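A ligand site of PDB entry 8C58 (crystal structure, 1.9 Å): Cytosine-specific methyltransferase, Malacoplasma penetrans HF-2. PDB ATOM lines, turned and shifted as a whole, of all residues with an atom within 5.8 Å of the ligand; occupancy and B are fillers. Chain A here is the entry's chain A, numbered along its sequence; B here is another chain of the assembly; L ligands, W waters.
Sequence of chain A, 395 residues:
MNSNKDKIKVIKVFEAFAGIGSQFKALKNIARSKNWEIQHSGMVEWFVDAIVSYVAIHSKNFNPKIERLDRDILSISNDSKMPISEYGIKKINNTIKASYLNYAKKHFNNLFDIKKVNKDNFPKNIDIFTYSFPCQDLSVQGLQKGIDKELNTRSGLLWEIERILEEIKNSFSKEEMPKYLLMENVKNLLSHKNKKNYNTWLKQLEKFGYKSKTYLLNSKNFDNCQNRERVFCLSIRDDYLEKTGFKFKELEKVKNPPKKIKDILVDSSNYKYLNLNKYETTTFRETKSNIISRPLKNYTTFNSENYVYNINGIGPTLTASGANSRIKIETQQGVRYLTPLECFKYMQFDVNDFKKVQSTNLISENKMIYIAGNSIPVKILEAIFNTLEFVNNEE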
ATOM      1  N   GLU A  15      12.380 -12.827 -14.411  1.00  0.00           N
ATOM      2  CA  GLU A  15      13.101 -13.315 -15.572  1.00  0.00           C
ATOM      3  C   GLU A  15      12.977 -12.347 -16.742  1.00  0.00           C
ATOM      4  O   GLU A  15      11.932 -12.306 -17.382  1.00  0.00           O
ATOM      5  CB  GLU A  15      12.537 -14.673 -16.016  1.00  0.00           C
ATOM      6  CG  GLU A  15      12.703 -15.813 -15.041  1.00  0.00           C
ATOM      7  CD  GLU A  15      11.866 -17.021 -15.429  1.00  0.00           C
ATOM      8  OE1 GLU A  15      10.663 -17.031 -15.086  1.00  0.00           O
ATOM      9  OE2 GLU A  15      12.424 -17.967 -16.069  1.00  0.00           O
ATOM     10  N   PHE A  17      13.822 -11.379 -20.529  1.00  0.00           N
ATOM     11  CA  PHE A  17      14.087 -12.191 -21.740  1.00  0.00           C
ATOM     12  C   PHE A  17      13.929 -13.667 -21.400  1.00  0.00           C
ATOM     13  O   PHE A  17      14.835 -14.495 -21.618  1.00  0.00           O
ATOM     14  CB  PHE A  17      15.455 -11.847 -22.329  1.00  0.00           C
ATOM     15  CG  PHE A  17      15.727 -10.372 -22.358  1.00  0.00           C
ATOM     16  CD1 PHE A  17      14.869  -9.512 -22.998  1.00  0.00           C
ATOM     17  CD2 PHE A  17      16.830  -9.845 -21.700  1.00  0.00           C
ATOM     18  CE1 PHE A  17      15.093  -8.141 -23.001  1.00  0.00           C
ATOM     19  CE2 PHE A  17      17.074  -8.480 -21.714  1.00  0.00           C
ATOM     20  CZ  PHE A  17      16.206  -7.631 -22.356  1.00  0.00           C
ATOM     21  N   ALA A  18      12.752 -13.989 -20.854  1.00  0.00           N
ATOM     22  CA  ALA A  18      12.530 -15.244 -20.163  1.00  0.00           C
ATOM     23  C   ALA A  18      12.517 -16.485 -21.036  1.00  0.00           C
ATOM     24  O   ALA A  18      12.819 -17.573 -20.555  1.00  0.00           O
ATOM     25  CB  ALA A  18      11.232 -15.174 -19.366  1.00  0.00           C
ATOM     26  N   GLY A  19      12.171 -16.333 -22.321  1.00  0.00           N
ATOM     27  CA  GLY A  19      11.997 -17.461 -23.212  1.00  0.00           C
ATOM     28  C   GLY A  19      10.988 -18.453 -22.677  1.00  0.00           C
ATOM     29  O   GLY A  19       9.862 -18.073 -22.304  1.00  0.00           O
ATOM     30  N   ILE A  20      11.397 -19.716 -22.589  1.00  0.00           N
ATOM     31  CA  ILE A  20      10.555 -20.770 -22.040  1.00  0.00           C
ATOM     32  C   ILE A  20      10.813 -21.058 -20.564  1.00  0.00           C
ATOM     33  O   ILE A  20      10.298 -22.018 -20.009  1.00  0.00           O
ATOM     34  CB  ILE A  20      10.629 -22.056 -22.871  1.00  0.00           C
ATOM     35  CG1 ILE A  20      12.078 -22.547 -23.011  1.00  0.00           C
ATOM     36  CG2 ILE A  20      10.018 -21.793 -24.233  1.00  0.00           C
ATOM     37  CD1 ILE A  20      12.166 -23.946 -23.591  1.00  0.00           C
ATOM     38  N   GLY A  21      11.616 -20.210 -19.943  1.00  0.00           N
ATOM     39  CA  GLY A  21      11.793 -20.261 -18.509  1.00  0.00           C
ATOM     40  C   GLY A  21      12.733 -21.338 -18.003  1.00  0.00           C
ATOM     41  O   GLY A  21      12.401 -22.036 -17.045  1.00  0.00           O
ATOM     42  N   SER A  22      13.906 -21.491 -18.619  1.00  0.00           N
ATOM     43  CA  SER A  22      14.898 -22.437 -18.095  1.00  0.00           C
ATOM     44  C   SER A  22      15.289 -22.059 -16.669  1.00  0.00           C
ATOM     45  O   SER A  22      15.547 -22.931 -15.847  1.00  0.00           O
ATOM     46  CB  SER A  22      16.137 -22.504 -18.986  1.00  0.00           C
ATOM     47  OG  SER A  22      16.750 -21.228 -19.131  1.00  0.00           O
ATOM     48  N   GLN A  23      15.314 -20.752 -16.396  1.00  0.00           N
ATOM     49  CA  GLN A  23      15.679 -20.220 -15.080  1.00  0.00           C
ATOM     50  C   GLN A  23      14.643 -20.682 -14.042  1.00  0.00           C
ATOM     51  O   GLN A  23      14.997 -21.250 -13.012  1.00  0.00           O
ATOM     52  CB  GLN A  23      15.760 -18.689 -15.084  1.00  0.00           C
ATOM     53  CG  GLN A  23      16.666 -18.063 -16.141  1.00  0.00           C
ATOM     54  CD  GLN A  23      16.064 -17.933 -17.543  1.00  0.00           C
ATOM     55  OE1 GLN A  23      16.805 -17.830 -18.517  1.00  0.00           O
ATOM     56  NE2 GLN A  23      14.729 -17.940 -17.654  1.00  0.00           N
ATOM     57  N   VAL A  44       9.737 -10.703 -18.480  1.00  0.00           N
ATOM     58  CA  VAL A  44       9.687  -9.890 -19.674  1.00  0.00           C
ATOM     59  C   VAL A  44       9.982 -10.788 -20.853  1.00  0.00           C
ATOM     60  O   VAL A  44      11.101 -11.296 -20.995  1.00  0.00           O
ATOM     61  CB  VAL A  44      10.703  -8.742 -19.613  1.00  0.00           C
ATOM     62  CG1 VAL A  44      10.477  -7.793 -20.769  1.00  0.00           C
ATOM     63  CG2 VAL A  44      10.606  -8.001 -18.294  1.00  0.00           C
ATOM     64  N   GLU A  45       8.972 -11.029 -21.671  1.00  0.00           N
ATOM     65  CA  GLU A  45       9.147 -11.820 -22.876  1.00  0.00           C
ATOM     66  C   GLU A  45       8.075 -11.429 -23.877  1.00  0.00           C
ATOM     67  O   GLU A  45       6.893 -11.462 -23.562  1.00  0.00           O
ATOM     68  CB  GLU A  45       9.065 -13.327 -22.573  1.00  0.00           C
ATOM     69  CG  GLU A  45       9.221 -14.230 -23.796  1.00  0.00           C
ATOM     70  CD  GLU A  45      10.470 -13.936 -24.602  1.00  0.00           C
ATOM     71  OE1 GLU A  45      11.593 -14.208 -24.106  1.00  0.00           O
ATOM     72  OE2 GLU A  45      10.357 -13.427 -25.736  1.00  0.00           O
ATOM     73  N   TRP A  46       8.501 -11.037 -25.064  1.00  0.00           N
ATOM     74  CA  TRP A  46       7.583 -10.523 -26.076  1.00  0.00           C
ATOM     75  C   TRP A  46       7.278 -11.473 -27.237  1.00  0.00           C
ATOM     76  O   TRP A  46       6.410 -11.193 -28.062  1.00  0.00           O
ATOM     77  CB  TRP A  46       8.110  -9.197 -26.624  1.00  0.00           C
ATOM     78  CG  TRP A  46       9.150  -9.270 -27.690  1.00  0.00           C
ATOM     79  CD1 TRP A  46      10.100 -10.238 -27.869  1.00  0.00           C
ATOM     80  CD2 TRP A  46       9.372  -8.307 -28.708  1.00  0.00           C
ATOM     81  NE1 TRP A  46      10.877  -9.937 -28.967  1.00  0.00           N
ATOM     82  CE2 TRP A  46      10.444  -8.748 -29.491  1.00  0.00           C
ATOM     83  CE3 TRP A  46       8.744  -7.095 -29.042  1.00  0.00           C
ATOM     84  CZ2 TRP A  46      10.925  -8.031 -30.598  1.00  0.00           C
ATOM     85  CZ3 TRP A  46       9.212  -6.376 -30.146  1.00  0.00           C
ATOM     86  CH2 TRP A  46      10.289  -6.854 -30.910  1.00  0.00           C
ATOM     87  N   PHE A  47       8.010 -12.583 -27.300  1.00  0.00           N
ATOM     88  CA  PHE A  47       7.900 -13.559 -28.404  1.00  0.00           C
ATOM     89  C   PHE A  47       6.707 -14.480 -28.181  1.00  0.00           C
ATOM     90  O   PHE A  47       6.702 -15.311 -27.276  1.00  0.00           O
ATOM     91  CB  PHE A  47       9.220 -14.330 -28.462  1.00  0.00           C
ATOM     92  CG  PHE A  47       9.334 -15.382 -29.546  1.00  0.00           C
ATOM     93  CD1 PHE A  47       8.612 -15.309 -30.724  1.00  0.00           C
ATOM     94  CD2 PHE A  47      10.262 -16.416 -29.390  1.00  0.00           C
ATOM     95  CE1 PHE A  47       8.756 -16.283 -31.704  1.00  0.00           C
ATOM     96  CE2 PHE A  47      10.415 -17.388 -30.365  1.00  0.00           C
ATOM     97  CZ  PHE A  47       9.658 -17.317 -31.527  1.00  0.00           C
ATOM     98  N   ALA A  50       7.192 -18.223 -27.525  1.00  0.00           N
ATOM     99  CA  ALA A  50       7.846 -18.444 -26.241  1.00  0.00           C
ATOM    100  C   ALA A  50       6.855 -18.238 -25.095  1.00  0.00           C
ATOM    101  O   ALA A  50       6.863 -19.014 -24.127  1.00  0.00           O
ATOM    102  CB  ALA A  50       9.042 -17.537 -26.069  1.00  0.00           C
ATOM    103  N   SER A  80      10.261 -12.967 -32.900  1.00  0.00           N
ATOM    104  CA  SER A  80      11.212 -12.688 -31.791  1.00  0.00           C
ATOM    105  C   SER A  80      12.127 -11.482 -32.058  1.00  0.00           C
ATOM    106  O   SER A  80      12.780 -10.981 -31.135  1.00  0.00           O
ATOM    107  CB  SER A  80      12.063 -13.921 -31.410  1.00  0.00           C
ATOM    108  OG  SER A  80      13.207 -14.058 -32.247  1.00  0.00           O
ATOM    109  N   PHE A 112       6.193  -7.926 -20.951  1.00  0.00           N
ATOM    110  CA  PHE A 112       6.299  -8.133 -22.414  1.00  0.00           C
ATOM    111  C   PHE A 112       7.535  -7.534 -23.063  1.00  0.00           C
ATOM    112  O   PHE A 112       8.353  -8.270 -23.600  1.00  0.00           O
ATOM    113  CB  PHE A 112       5.023  -7.724 -23.152  1.00  0.00           C
ATOM    114  CG  PHE A 112       3.836  -8.585 -22.822  1.00  0.00           C
ATOM    115  CD1 PHE A 112       3.603  -9.762 -23.513  1.00  0.00           C
ATOM    116  CD2 PHE A 112       2.974  -8.243 -21.799  1.00  0.00           C
ATOM    117  CE1 PHE A 112       2.532 -10.571 -23.189  1.00  0.00           C
ATOM    118  CE2 PHE A 112       1.898  -9.038 -21.471  1.00  0.00           C
ATOM    119  CZ  PHE A 112       1.674 -10.205 -22.160  1.00  0.00           C
ATOM    120  N   ASP A 113       7.676  -6.226 -22.995  1.00  0.00           N
ATOM    121  CA  ASP A 113       8.737  -5.514 -23.697  1.00  0.00           C
ATOM    122  C   ASP A 113       9.588  -4.787 -22.668  1.00  0.00           C
ATOM    123  O   ASP A 113       9.062  -4.019 -21.865  1.00  0.00           O
ATOM    124  CB  ASP A 113       8.076  -4.517 -24.646  1.00  0.00           C
ATOM    125  CG  ASP A 113       9.063  -3.784 -25.538  1.00  0.00           C
ATOM    126  OD1 ASP A 113      10.288  -3.898 -25.374  1.00  0.00           O
ATOM    127  OD2 ASP A 113       8.551  -3.049 -26.413  1.00  0.00           O
ATOM    128  N   ILE A 114      10.897  -5.025 -22.703  1.00  0.00           N
ATOM    129  CA  ILE A 114      11.820  -4.414 -21.743  1.00  0.00           C
ATOM    130  C   ILE A 114      11.787  -2.883 -21.774  1.00  0.00           C
ATOM    131  O   ILE A 114      11.973  -2.230 -20.749  1.00  0.00           O
ATOM    132  CB  ILE A 114      13.266  -4.945 -21.906  1.00  0.00           C
ATOM    133  CG1 ILE A 114      14.122  -4.615 -20.678  1.00  0.00           C
ATOM    134  CG2 ILE A 114      13.920  -4.387 -23.173  1.00  0.00           C
ATOM    135  CD1 ILE A 114      13.823  -5.485 -19.483  1.00  0.00           C
ATOM    136  N   LYS A 115      11.491  -2.304 -22.936  1.00  0.00           N
ATOM    137  CA  LYS A 115      11.359  -0.841 -23.058  1.00  0.00           C
ATOM    138  C   LYS A 115      10.197  -0.272 -22.238  1.00  0.00           C
ATOM    139  O   LYS A 115      10.182   0.932 -21.936  1.00  0.00           O
ATOM    140  CB  LYS A 115      11.223  -0.423 -24.531  1.00  0.00           C
ATOM    141  CG  LYS A 115      12.390  -0.835 -25.415  1.00  0.00           C
ATOM    142  CD  LYS A 115      12.198  -0.382 -26.864  1.00  0.00           C
ATOM    143  CE  LYS A 115      13.461  -0.557 -27.693  1.00  0.00           C
ATOM    144  NZ  LYS A 115      14.183  -1.853 -27.451  1.00  0.00           N
ATOM    145  N   LEU A 157      19.067  -3.607 -25.763  1.00  0.00           N
ATOM    146  CA  LEU A 157      18.529  -4.296 -24.592  1.00  0.00           C
ATOM    147  C   LEU A 157      19.314  -4.026 -23.311  1.00  0.00           C
ATOM    148  O   LEU A 157      18.724  -3.956 -22.241  1.00  0.00           O
ATOM    149  CB  LEU A 157      18.452  -5.799 -24.829  1.00  0.00           C
ATOM    150  CG  LEU A 157      17.224  -6.336 -25.569  1.00  0.00           C
ATOM    151  CD1 LEU A 157      16.908  -5.561 -26.841  1.00  0.00           C
ATOM    152  CD2 LEU A 157      17.446  -7.803 -25.873  1.00  0.00           C
ATOM    153  N   GLU A 184      23.128 -14.557 -18.673  1.00  0.00           N
ATOM    154  CA  GLU A 184      23.642 -15.624 -19.537  1.00  0.00           C
ATOM    155  C   GLU A 184      23.939 -14.990 -20.879  1.00  0.00           C
ATOM    156  O   GLU A 184      23.245 -14.064 -21.304  1.00  0.00           O
ATOM    157  CB  GLU A 184      22.615 -16.760 -19.714  1.00  0.00           C
ATOM    158  CG  GLU A 184      23.037 -17.857 -20.707  1.00  0.00           C
ATOM    159  CD  GLU A 184      22.488 -17.686 -22.129  1.00  0.00           C
ATOM    160  OE1 GLU A 184      21.723 -16.720 -22.375  1.00  0.00           O
ATOM    161  OE2 GLU A 184      22.792 -18.539 -23.011  1.00  0.00           O
ATOM    162  N   PHE A 349      15.199 -29.986 -20.340  1.00  0.00           N
ATOM    163  CA  PHE A 349      13.782 -29.960 -20.006  1.00  0.00           C
ATOM    164  C   PHE A 349      13.334 -31.407 -19.971  1.00  0.00           C
ATOM    165  O   PHE A 349      14.059 -32.271 -20.441  1.00  0.00           O
ATOM    166  CB  PHE A 349      12.998 -29.127 -21.022  1.00  0.00           C
ATOM    167  CG  PHE A 349      13.178 -27.649 -20.831  1.00  0.00           C
ATOM    168  CD1 PHE A 349      14.280 -26.996 -21.338  1.00  0.00           C
ATOM    169  CD2 PHE A 349      12.274 -26.922 -20.079  1.00  0.00           C
ATOM    170  CE1 PHE A 349      14.465 -25.645 -21.141  1.00  0.00           C
ATOM    171  CE2 PHE A 349      12.440 -25.556 -19.876  1.00  0.00           C
ATOM    172  CZ  PHE A 349      13.549 -24.924 -20.408  1.00  0.00           C
ATOM    173  N   ILE A 371      12.719 -22.343 -29.980  1.00  0.00           N
ATOM    174  CA  ILE A 371      12.659 -21.939 -28.581  1.00  0.00           C
ATOM    175  C   ILE A 371      13.581 -22.765 -27.692  1.00  0.00           C
ATOM    176  O   ILE A 371      14.183 -22.218 -26.772  1.00  0.00           O
ATOM    177  CB  ILE A 371      11.203 -21.874 -28.007  1.00  0.00           C
ATOM    178  CG1 ILE A 371      10.522 -23.248 -27.997  1.00  0.00           C
ATOM    179  CG2 ILE A 371      10.409 -20.896 -28.834  1.00  0.00           C
ATOM    180  CD1 ILE A 371       9.078 -23.235 -27.560  1.00  0.00           C
ATOM    181  N   ASN A 374      17.143 -21.441 -28.235  1.00  0.00           N
ATOM    182  CA  ASN A 374      17.337 -20.193 -27.537  1.00  0.00           C
ATOM    183  C   ASN A 374      17.483 -20.307 -26.019  1.00  0.00           C
ATOM    184  O   ASN A 374      17.867 -19.338 -25.367  1.00  0.00           O
ATOM    185  CB  ASN A 374      16.138 -19.257 -27.787  1.00  0.00           C
ATOM    186  CG  ASN A 374      16.293 -18.398 -29.014  1.00  0.00           C
ATOM    187  OD1 ASN A 374      17.392 -18.178 -29.506  1.00  0.00           O
ATOM    188  ND2 ASN A 374      15.184 -17.834 -29.470  1.00  0.00           N
ATOM    189  N   SER A 375      17.185 -21.475 -25.457  1.00  0.00           N
ATOM    190  CA  SER A 375      17.157 -21.653 -24.007  1.00  0.00           C
ATOM    191  C   SER A 375      18.529 -21.967 -23.424  1.00  0.00           C
ATOM    192  O   SER A 375      19.540 -21.865 -24.108  1.00  0.00           O
ATOM    193  CB  SER A 375      16.147 -22.739 -23.638  1.00  0.00           C
ATOM    194  OG  SER A 375      15.755 -22.614 -22.288  1.00  0.00           O
ATOM    195  N   ILE A 376      18.561 -22.319 -22.142  1.00  0.00           N
ATOM    196  CA  ILE A 376      19.786 -22.614 -21.424  1.00  0.00           C
ATOM    197  C   ILE A 376      19.680 -24.000 -20.829  1.00  0.00           C
ATOM    198  O   ILE A 376      18.669 -24.319 -20.208  1.00  0.00           O
ATOM    199  CB  ILE A 376      19.974 -21.622 -20.259  1.00  0.00           C
ATOM    200  CG1 ILE A 376      19.887 -20.177 -20.769  1.00  0.00           C
ATOM    201  CG2 ILE A 376      21.300 -21.907 -19.552  1.00  0.00           C
ATOM    202  CD1 ILE A 376      19.886 -19.125 -19.657  1.00  0.00           C
ATOM    203  P   5OC B   8      26.560 -20.316 -30.537  1.00  0.00           P
ATOM    204  N1  5OC B   8      21.421 -18.376 -27.760  1.00  0.00           N
ATOM    205  C2  5OC B   8      21.800 -18.667 -26.496  1.00  0.00           C
ATOM    206  O2  5OC B   8      22.060 -19.812 -26.123  1.00  0.00           O
ATOM    207  N3  5OC B   8      21.923 -17.654 -25.552  1.00  0.00           N
ATOM    208  C4  5OC B   8      21.697 -16.327 -25.889  1.00  0.00           C
ATOM    209  N4  5OC B   8      21.820 -15.354 -24.993  1.00  0.00           N
ATOM    210  C5  5OC B   8      21.333 -15.987 -27.190  1.00  0.00           C
ATOM    211  O5  5OC B   8      21.111 -14.669 -27.493  1.00  0.00           O
ATOM    212  C6  5OC B   8      21.209 -17.009 -28.130  1.00  0.00           C
ATOM    213  C1' 5OC B   8      21.336 -19.471 -28.745  1.00  0.00           C
ATOM    214  C2' 5OC B   8      20.555 -19.168 -30.036  1.00  0.00           C
ATOM    215  C3' 5OC B   8      21.598 -19.089 -31.125  1.00  0.00           C
ATOM    216  O3' 5OC B   8      21.107 -19.762 -32.302  1.00  0.00           O
ATOM    217  C4' 5OC B   8      22.687 -19.962 -30.526  1.00  0.00           C
ATOM    218  O4' 5OC B   8      22.685 -19.633 -29.145  1.00  0.00           O
ATOM    219  C5' 5OC B   8      24.072 -19.649 -31.078  1.00  0.00           C
ATOM    220  O5' 5OC B   8      24.982 -20.606 -30.516  1.00  0.00           O
ATOM    221  OP1 5OC B   8      26.818 -18.875 -30.573  1.00  0.00           O
ATOM    222  OP2 5OC B   8      27.113 -21.142 -29.439  1.00  0.00           O
HETATM  223  N1  LIG L   1      16.848 -17.753 -21.423  1.00  0.00           N
HETATM  224  C1  LIG L   1      15.611 -17.941 -22.176  1.00  0.00           C
HETATM  225  C2  LIG L   1      15.051 -19.339 -21.916  1.00  0.00           C
HETATM  226  O1  LIG L   1      15.187 -19.830 -20.786  1.00  0.00           O
HETATM  227  O2  LIG L   1      14.435 -19.986 -22.790  1.00  0.00           O
HETATM  228  C3  LIG L   1      15.824 -17.643 -23.664  1.00  0.00           C
HETATM  229  C4  LIG L   1      16.476 -16.270 -23.913  1.00  0.00           C
HETATM  230  S1  LIG L   1      16.535 -15.835 -25.529  1.00  0.00           S
HETATM  231  C5  LIG L   1      18.037 -16.202 -26.161  1.00  0.00           C
HETATM  232  C6  LIG L   1      16.313 -14.181 -25.705  1.00  0.00           C
HETATM  233  C7  LIG L   1      14.828 -13.805 -25.593  1.00  0.00           C
HETATM  234  O3  LIG L   1      14.673 -12.394 -25.515  1.00  0.00           O
HETATM  235  C8  LIG L   1      13.988 -14.270 -26.778  1.00  0.00           C
HETATM  236  O4  LIG L   1      13.011 -15.200 -26.272  1.00  0.00           O
HETATM  237  C9  LIG L   1      13.390 -12.981 -27.329  1.00  0.00           C
HETATM  238  O5  LIG L   1      12.050 -13.126 -27.759  1.00  0.00           O
HETATM  239  C10 LIG L   1      13.444 -12.035 -26.147  1.00  0.00           C
HETATM  240  N2  LIG L   1      13.418 -10.604 -26.505  1.00  0.00           N
HETATM  241  C11 LIG L   1      14.062  -9.964 -27.493  1.00  0.00           C
HETATM  242  N3  LIG L   1      13.768  -8.639 -27.475  1.00  0.00           N
HETATM  243  C12 LIG L   1      12.898  -8.430 -26.466  1.00  0.00           C
HETATM  244  C13 LIG L   1      12.178  -7.288 -25.879  1.00  0.00           C
HETATM  245  N4  LIG L   1      12.303  -6.038 -26.377  1.00  0.00           N
HETATM  246  N5  LIG L   1      11.389  -7.525 -24.816  1.00  0.00           N
HETATM  247  C14 LIG L   1      11.232  -8.757 -24.309  1.00  0.00           C
HETATM  248  N6  LIG L   1      11.839  -9.846 -24.804  1.00  0.00           N
HETATM  249  C15 LIG L   1      12.679  -9.732 -25.843  1.00  0.00           C
HETATM  250  O   HOH W   1      13.529 -19.877 -25.387  1.00  0.00           O
HETATM  251  O   HOH W   2      19.200 -18.170 -23.185  1.00  0.00           O
HETATM  252  O   HOH W   3      12.813 -17.826 -27.314  1.00  0.00           O
HETATM  253  O   HOH W   4      16.375 -13.319 -29.112  1.00  0.00           O
HETATM  254  O   HOH W   5      19.041 -15.756 -21.204  1.00  0.00           O
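An oxygen (O1) of the ligand sits close to the backbone carbonyl oxygen (O) of Ala 18 (3.3 Å). N5 of the ligand sits close to O of Phe 112. The backbone carbonyl oxygen of Asn 374 lies close to a sulfur (S1) of the ligand, at 3.8 Å. Phe 17 touches the ligand (CB to O3, 3.3 Å). CA of Gly 19 touches O2 of the ligand, 3.5 Å away. N of Gly 21 touches O1 of the ligand (3.7 Å). Val 44 touches the ligand. Trp 46 touches the ligand. CB of Phe 47 touches O5 of the ligand (3.2 Å). Ser 80 touches the ligand. CD1 of Ile 376 touches N1 of the ligand (3.8 Å). 5OC 8 of chain B touches the ligand. Hydrophobic or aromatic side chains that line the ligand: Phe 17, Ile 20, Val 44, Trp 46, Phe 47, Ile 114 and Ile 376. 19 residues have an atom within 4 Å of the ligand: Phe 17, Ala 18, Gly 19, Ile 20, Gly 21, Ser 22, Gln 23, Val 44, Glu 45, Trp 46, Phe 47, Ser 80, Phe 112, Asp 113, Ile 114, Asn 374, Ser 375, Ile 376 and 5OC 8 of chain B. The nearest printed residue that does not touch the ligand is Leu 157 (4.1 Å).
The side-chain hydroxyl (OG) of Ser 375 is in hydrogen-bond range of an oxygen (O2) of the ligand, at 3.0 Å. OE2 of Glu 45 lies within hydrogen-bond range of O5 of the ligand (2.7 Å). The side-chain amide oxygen (OE1) of Gln 23 lies within hydrogen-bond range of a nitrogen (N1) of the ligand, 2.9 Å away. N of Ile 20 lies within hydrogen-bond range of O2 of the ligand (3.1 Å). N of Ile 114 sits at hydrogen-bond distance from N5 of the ligand (3.3 Å). OG of Ser 22 sits at hydrogen-bond distance from O1 of the ligand (2.7 Å). The side-chain carboxylate of Asp 113 lies within hydrogen-bond range of a nitrogen (N4) of the ligand (3.1 Å). O1 of the ligand sits at hydrogen-bond distance from N of Ser 22, at 3.0 Å.
Water W1 lies within hydrogen-bond range of O2 of the ligand (2.8 Å) and O of Ile 371 (2.8 Å). Water W3 lies within hydrogen-bond range of O4 of the ligand and ND2 of Asn 374. Water W2 lies within hydrogen-bond range of the backbone carbonyl oxygen (O) of Asn 374, a nitrogen (N1) of the ligand and the side-chain carboxylate (OE1) of Glu 184. Water W5 lies within hydrogen-bond range of N1 of the ligand (3.0 Å) and OE1 of Glu 184 (3.1 Å).
OD1 of Asp 113 sits close to N of Lys 115 (3.2 Å). OE1 of Gln 23 is in hydrogen-bond range of OG of Ser 22, at 3.5 Å. The backbone NH (N) of Val 44 sits at hydrogen-bond distance from the backbone carbonyl oxygen (O) of Glu 15, 2.9 Å away. The side-chain amide nitrogen of Gln 23 lies within hydrogen-bond range of the backbone carbonyl oxygen of Ala 18 (3.5 Å). The backbone carbonyl oxygen (O) of Ser 80 lies within hydrogen-bond range of the indole nitrogen (NE1) of Trp 46, at 3.1 Å. The backbone carbonyl oxygen (O) of Phe 112 lies within hydrogen-bond range of the backbone NH (N) of Trp 46. The side-chain carboxylate (OE2) of Glu 45 lies within hydrogen-bond range of the backbone NH (N) of Phe 47 (2.9 Å). The backbone NH (N) of Ala 18 is in hydrogen-bond range of the backbone carbonyl oxygen (O) of Val 44 (3.2 Å).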
